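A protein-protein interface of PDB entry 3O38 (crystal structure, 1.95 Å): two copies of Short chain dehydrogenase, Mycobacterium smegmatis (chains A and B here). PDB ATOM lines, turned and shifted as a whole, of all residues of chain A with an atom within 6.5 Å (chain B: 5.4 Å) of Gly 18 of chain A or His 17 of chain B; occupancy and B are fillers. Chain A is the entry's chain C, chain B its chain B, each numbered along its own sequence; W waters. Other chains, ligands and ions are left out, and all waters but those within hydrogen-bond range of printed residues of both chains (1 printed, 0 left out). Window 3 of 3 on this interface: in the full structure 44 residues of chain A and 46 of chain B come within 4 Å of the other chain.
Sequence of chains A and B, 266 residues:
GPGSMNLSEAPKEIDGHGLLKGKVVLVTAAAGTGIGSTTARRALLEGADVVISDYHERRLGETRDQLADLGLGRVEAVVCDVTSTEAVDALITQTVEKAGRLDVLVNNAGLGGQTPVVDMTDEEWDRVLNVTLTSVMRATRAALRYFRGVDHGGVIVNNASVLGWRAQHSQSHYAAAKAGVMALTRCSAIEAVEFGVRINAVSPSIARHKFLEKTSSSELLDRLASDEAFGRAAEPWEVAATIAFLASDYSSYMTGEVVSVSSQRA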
ATOM      1  N   GLY A  16      36.194  22.132  -0.650  1.00  0.00           N
ATOM      2  CA  GLY A  16      35.452  21.600  -1.789  1.00  0.00           C
ATOM      3  C   GLY A  16      34.352  20.640  -1.394  1.00  0.00           C
ATOM      4  O   GLY A  16      34.427  20.010  -0.354  1.00  0.00           O
ATOM      5  N   HIS A  17      33.321  20.533  -2.232  1.00  0.00           N
ATOM      6  CA  HIS A  17      32.181  19.649  -1.972  1.00  0.00           C
ATOM      7  C   HIS A  17      31.843  18.846  -3.214  1.00  0.00           C
ATOM      8  O   HIS A  17      30.717  18.450  -3.381  1.00  0.00           O
ATOM      9  CB  HIS A  17      30.954  20.442  -1.448  1.00  0.00           C
ATOM     10  CG  HIS A  17      31.168  21.028  -0.073  1.00  0.00           C
ATOM     11  ND1 HIS A  17      31.922  22.161   0.145  1.00  0.00           N
ATOM     12  CD2 HIS A  17      30.795  20.589   1.151  1.00  0.00           C
ATOM     13  CE1 HIS A  17      31.981  22.417   1.442  1.00  0.00           C
ATOM     14  NE2 HIS A  17      31.297  21.481   2.074  1.00  0.00           N
ATOM     15  N   GLY A  18      32.833  18.620  -4.074  1.00  0.00           N
ATOM     16  CA  GLY A  18      32.660  17.815  -5.283  1.00  0.00           C
ATOM     17  C   GLY A  18      31.700  18.338  -6.367  1.00  0.00           C
ATOM     18  O   GLY A  18      31.199  17.550  -7.171  1.00  0.00           O
ATOM     19  N   LEU A  19      31.476  19.656  -6.417  1.00  0.00           N
ATOM     20  CA  LEU A  19      30.483  20.240  -7.326  1.00  0.00           C
ATOM     21  C   LEU A  19      30.822  20.133  -8.839  1.00  0.00           C
ATOM     22  O   LEU A  19      29.933  20.156  -9.688  1.00  0.00           O
ATOM     23  CB  LEU A  19      30.213  21.710  -6.953  1.00  0.00           C
ATOM     24  CG  LEU A  19      29.781  22.110  -5.527  1.00  0.00           C
ATOM     25  CD1 LEU A  19      29.401  23.583  -5.502  1.00  0.00           C
ATOM     26  CD2 LEU A  19      28.616  21.264  -5.034  1.00  0.00           C
ATOM     27  N   LEU A  20      32.103  20.045  -9.157  1.00  0.00           N
ATOM     28  CA  LEU A  20      32.553  19.967 -10.563  1.00  0.00           C
ATOM     29  C   LEU A  20      33.435  18.724 -10.828  1.00  0.00           C
ATOM     30  O   LEU A  20      34.286  18.717 -11.743  1.00  0.00           O
ATOM     31  CB  LEU A  20      33.316  21.244 -10.942  1.00  0.00           C
ATOM     32  CG  LEU A  20      32.516  22.539 -10.735  1.00  0.00           C
ATOM     33  CD1 LEU A  20      33.468  23.723 -10.798  1.00  0.00           C
ATOM     34  CD2 LEU A  20      31.397  22.658 -11.761  1.00  0.00           C
ATOM     35  N   LYS A  21      33.208  17.676 -10.041  1.00  0.00           N
ATOM     36  CA  LYS A  21      34.033  16.473 -10.121  1.00  0.00           C
ATOM     37  C   LYS A  21      34.054  15.972 -11.562  1.00  0.00           C
ATOM     38  O   LYS A  21      33.011  15.697 -12.152  1.00  0.00           O
ATOM     39  CB  LYS A  21      33.583  15.409  -9.088  1.00  0.00           C
ATOM     40  N   LEU A  45      39.373  22.709  -6.116  1.00  0.00           N
ATOM     41  CA  LEU A  45      38.811  22.255  -4.848  1.00  0.00           C
ATOM     42  C   LEU A  45      37.507  21.469  -5.085  1.00  0.00           C
ATOM     43  O   LEU A  45      37.209  20.514  -4.338  1.00  0.00           O
ATOM     44  CB  LEU A  45      38.567  23.425  -3.891  1.00  0.00           C
ATOM     45  CG  LEU A  45      39.783  24.215  -3.383  1.00  0.00           C
ATOM     46  CD1 LEU A  45      39.317  25.506  -2.674  1.00  0.00           C
ATOM     47  CD2 LEU A  45      40.686  23.401  -2.428  1.00  0.00           C
ATOM     48  N   GLU A  46      36.767  21.848  -6.138  1.00  0.00           N
ATOM     49  CA  GLU A  46      35.527  21.139  -6.511  1.00  0.00           C
ATOM     50  C   GLU A  46      35.703  19.874  -7.378  1.00  0.00           C
ATOM     51  O   GLU A  46      34.711  19.312  -7.843  1.00  0.00           O
ATOM     52  CB  GLU A  46      34.514  22.104  -7.177  1.00  0.00           C
ATOM     53  CG  GLU A  46      34.047  23.260  -6.281  1.00  0.00           C
ATOM     54  CD  GLU A  46      33.498  22.842  -4.916  1.00  0.00           C
ATOM     55  OE1 GLU A  46      32.886  21.751  -4.781  1.00  0.00           O
ATOM     56  OE2 GLU A  46      33.661  23.629  -3.973  1.00  0.00           O
ATOM     57  N   GLY A  47      36.945  19.413  -7.568  1.00  0.00           N
ATOM     58  CA  GLY A  47      37.212  18.172  -8.313  1.00  0.00           C
ATOM     59  C   GLY A  47      37.463  18.287  -9.808  1.00  0.00           C
ATOM     60  O   GLY A  47      37.585  17.281 -10.515  1.00  0.00           O
ATOM     61  N   TYR A 250      23.744  22.616  -9.367  1.00  0.00           N
ATOM     62  CA  TYR A 250      22.829  23.254  -8.410  1.00  0.00           C
ATOM     63  C   TYR A 250      22.074  24.416  -9.078  1.00  0.00           C
ATOM     64  O   TYR A 250      21.046  24.773  -8.675  1.00  0.00           O
ATOM     65  CB  TYR A 250      23.510  23.635  -7.105  1.00  0.00           C
ATOM     66  CG  TYR A 250      23.818  22.447  -6.208  1.00  0.00           C
ATOM     67  CD1 TYR A 250      24.938  21.671  -6.408  1.00  0.00           C
ATOM     68  CD2 TYR A 250      22.978  22.102  -5.177  1.00  0.00           C
ATOM     69  CE1 TYR A 250      25.207  20.613  -5.638  1.00  0.00           C
ATOM     70  CE2 TYR A 250      23.229  21.008  -4.392  1.00  0.00           C
ATOM     71  CZ  TYR A 250      24.351  20.264  -4.613  1.00  0.00           C
ATOM     72  OH  TYR A 250      24.634  19.222  -3.835  1.00  0.00           O
ATOM     73  N   ILE B  14      19.977  15.636  -8.637  1.00  0.00           N
ATOM     74  CA  ILE B  14      21.371  15.352  -8.266  1.00  0.00           C
ATOM     75  C   ILE B  14      21.536  14.827  -6.838  1.00  0.00           C
ATOM     76  O   ILE B  14      20.694  15.045  -5.978  1.00  0.00           O
ATOM     77  CB  ILE B  14      22.301  16.593  -8.495  1.00  0.00           C
ATOM     78  CG1 ILE B  14      21.868  17.786  -7.612  1.00  0.00           C
ATOM     79  CG2 ILE B  14      22.344  16.965  -9.990  1.00  0.00           C
ATOM     80  CD1 ILE B  14      22.609  19.065  -7.896  1.00  0.00           C
ATOM     81  N   ASP B  15      22.649  14.145  -6.595  1.00  0.00           N
ATOM     82  CA  ASP B  15      23.012  13.678  -5.284  1.00  0.00           C
ATOM     83  C   ASP B  15      23.256  14.861  -4.351  1.00  0.00           C
ATOM     84  O   ASP B  15      23.423  15.983  -4.825  1.00  0.00           O
ATOM     85  CB  ASP B  15      24.289  12.851  -5.401  1.00  0.00           C
ATOM     86  CG  ASP B  15      24.063  11.509  -6.135  1.00  0.00           C
ATOM     87  OD1 ASP B  15      22.898  11.112  -6.370  1.00  0.00           O
ATOM     88  OD2 ASP B  15      25.069  10.854  -6.461  1.00  0.00           O
ATOM     89  N   GLY B  16      23.285  14.601  -3.038  1.00  0.00           N
ATOM     90  CA  GLY B  16      23.766  15.581  -2.069  1.00  0.00           C
ATOM     91  C   GLY B  16      25.283  15.736  -2.124  1.00  0.00           C
ATOM     92  O   GLY B  16      25.989  14.852  -2.622  1.00  0.00           O
ATOM     93  N   HIS B  17      25.787  16.870  -1.637  1.00  0.00           N
ATOM     94  CA  HIS B  17      27.230  17.137  -1.641  1.00  0.00           C
ATOM     95  C   HIS B  17      27.651  17.754  -0.330  1.00  0.00           C
ATOM     96  O   HIS B  17      28.680  18.426  -0.249  1.00  0.00           O
ATOM     97  CB  HIS B  17      27.633  18.037  -2.819  1.00  0.00           C
ATOM     98  CG  HIS B  17      27.456  17.401  -4.163  1.00  0.00           C
ATOM     99  ND1 HIS B  17      26.229  17.306  -4.785  1.00  0.00           N
ATOM    100  CD2 HIS B  17      28.355  16.845  -5.013  1.00  0.00           C
ATOM    101  CE1 HIS B  17      26.378  16.713  -5.957  1.00  0.00           C
ATOM    102  NE2 HIS B  17      27.658  16.419  -6.113  1.00  0.00           N
ATOM    103  N   GLY B  18      26.863  17.518   0.713  1.00  0.00           N
ATOM    104  CA  GLY B  18      27.284  17.875   2.061  1.00  0.00           C
ATOM    105  C   GLY B  18      27.201  19.353   2.345  1.00  0.00           C
ATOM    106  O   GLY B  18      27.853  19.836   3.285  1.00  0.00           O
ATOM    107  N   LEU B  19      26.405  20.077   1.546  1.00  0.00           N
ATOM    108  CA  LEU B  19      26.335  21.552   1.656  1.00  0.00           C
ATOM    109  C   LEU B  19      25.790  22.083   2.982  1.00  0.00           C
ATOM    110  O   LEU B  19      26.013  23.256   3.324  1.00  0.00           O
ATOM    111  CB  LEU B  19      25.522  22.150   0.508  1.00  0.00           C
ATOM    112  CG  LEU B  19      26.065  21.871  -0.904  1.00  0.00           C
ATOM    113  CD1 LEU B  19      25.202  22.563  -1.980  1.00  0.00           C
ATOM    114  CD2 LEU B  19      27.481  22.323  -1.014  1.00  0.00           C
ATOM    115  N   ARG B  42      15.869  17.836  -0.221  1.00  0.00           N
ATOM    116  CA  ARG B  42      17.190  18.412  -0.566  1.00  0.00           C
ATOM    117  C   ARG B  42      18.042  18.728   0.662  1.00  0.00           C
ATOM    118  O   ARG B  42      19.228  18.378   0.717  1.00  0.00           O
ATOM    119  CB  ARG B  42      17.058  19.639  -1.487  1.00  0.00           C
ATOM    120  CG  ARG B  42      18.360  20.484  -1.628  1.00  0.00           C
ATOM    121  CD  ARG B  42      19.493  19.766  -2.405  1.00  0.00           C
ATOM    122  NE  ARG B  42      18.994  18.998  -3.541  1.00  0.00           N
ATOM    123  CZ  ARG B  42      19.672  18.007  -4.129  1.00  0.00           C
ATOM    124  NH1 ARG B  42      20.888  17.705  -3.691  1.00  0.00           N
ATOM    125  NH2 ARG B  42      19.145  17.322  -5.163  1.00  0.00           N
ATOM    126  N   LEU B  45      19.326  15.486   1.911  1.00  0.00           N
ATOM    127  CA  LEU B  45      20.355  15.027   0.967  1.00  0.00           C
ATOM    128  C   LEU B  45      21.715  15.691   1.219  1.00  0.00           C
ATOM    129  O   LEU B  45      22.765  15.060   1.015  1.00  0.00           O
ATOM    130  CB  LEU B  45      19.917  15.258  -0.484  1.00  0.00           C
ATOM    131  CG  LEU B  45      18.895  14.281  -1.132  1.00  0.00           C
ATOM    132  CD1 LEU B  45      18.491  14.742  -2.522  1.00  0.00           C
ATOM    133  CD2 LEU B  45      19.453  12.830  -1.197  1.00  0.00           C
ATOM    134  N   GLU B  46      21.671  16.952   1.666  1.00  0.00           N
ATOM    135  CA  GLU B  46      22.858  17.773   1.939  1.00  0.00           C
ATOM    136  C   GLU B  46      23.396  17.620   3.374  1.00  0.00           C
ATOM    137  O   GLU B  46      24.316  18.347   3.782  1.00  0.00           O
ATOM    138  CB  GLU B  46      22.545  19.269   1.675  1.00  0.00           C
ATOM    139  CG  GLU B  46      22.164  19.639   0.261  1.00  0.00           C
ATOM    140  CD  GLU B  46      23.153  19.120  -0.795  1.00  0.00           C
ATOM    141  OE1 GLU B  46      24.360  18.962  -0.480  1.00  0.00           O
ATOM    142  OE2 GLU B  46      22.711  18.891  -1.941  1.00  0.00           O
HETATM  143  O   HOH W   1      29.461  21.971   4.879  1.00  0.00           O
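Among the printed residues, pairs that only touch across the chains: His 17 of chain A with His 17 of chain B (3.2 Å), Tyr 250 of chain A with Leu 19 of chain B (3.5 Å), Tyr 250 of chain A with Asp 15 of chain B (3.6 Å), Gly 18 of chain A with His 17 of chain B (3.6 Å), His 17 of chain A with Gly 18 of chain B (3.7 Å), Tyr 250 of chain A with Ile 14 of chain B (3.8 Å), Tyr 250 of chain A with Gly 16 of chain B (3.9 Å) and His 17 of chain A with Leu 19 of chain B (3.97 Å).
His 17 of chain B touches its own counterpart, His 17 of chain A. His 17 of chain A touches Gly 18 of chain B, and with the chains exchanged Gly 18 of chain A touches His 17 of chain B. His 17 of chain A touches Leu 19 of chain B, but with the chains exchanged Leu 19 of chain A does not touch His 17 of chain B (4.04 Å). 6 positions are printed for both chains.
Hydrophobic or aromatic side chains of chain B that line the printed part of chain A: Ile 14, His 17 and Leu 19. Of the 10 printed residues of chain A, 3 touch a printed residue of chain B. Hydrophobic or aromatic side chains of chain A within 4 Å of the printed part of chain B: His 17 and Tyr 250. Among the printed residues, 10 pairs touch across the chains. Among the printed residues, no Asp or Glu carboxylate lies within 4 Å of a Lys or Arg side-chain nitrogen of the other chain.
N of Leu 19 of chain B sits at hydrogen-bond distance from OE1 of Glu 46 of chain B (3.1 Å). OE1 of Glu 46 of chain A sits at hydrogen-bond distance from N of His 17 of chain A (2.9 Å). The side-chain carboxylate (OE1) of Glu 46 of chain A is in hydrogen-bond range of the backbone NH (N) of Gly 18 of chain A (3.2 Å). N of Gly 18 of chain B sits at hydrogen-bond distance from OE1 of Glu 46 of chain B (3.1 Å). The backbone carbonyl oxygen (O) of Asp 15 of chain B is in hydrogen-bond range of a ring nitrogen (ND1) of His 17 of chain B, 3.1 Å away. The backbone carbonyl oxygen (O) of Ile 14 of chain B sits at hydrogen-bond distance from the guanidinium group (NH2) of Arg 42 of chain B (2.9 Å).
Of chain B, only His 17 (3.6 Å) comes within 4 Å of Gly 18 of chain A. Of the printed residues of chain A, Ile 14 of chain B touches Tyr 250 (3.8 Å). Printed residues of chain A within 4 Å of Gly 18 of chain B: His 17 (3.7 Å). Printed residues of chain A within 4 Å of Leu 19 of chain B: His 17 (3.97 Å) and Tyr 250 (3.5 Å). The nearest printed residue of chain B that does not touch Gly 18 of chain A is Leu 19 of chain B (7.2 Å). The nearest residue of chain A that does not touch His 17 of chain B is Leu 19 of chain A (4.04 Å).
Water W1 bridges O of Gly 18 of chain B (3.1 Å) and NE2 of His 17 of chain A (3.4 Å).
OH of Tyr 250 of chain A sits at hydrogen-bond distance from OE2 of Glu 46 of chain B. OH of Tyr 250 of chain A lies within hydrogen-bond range of ND1 of His 17 of chain B (2.7 Å).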
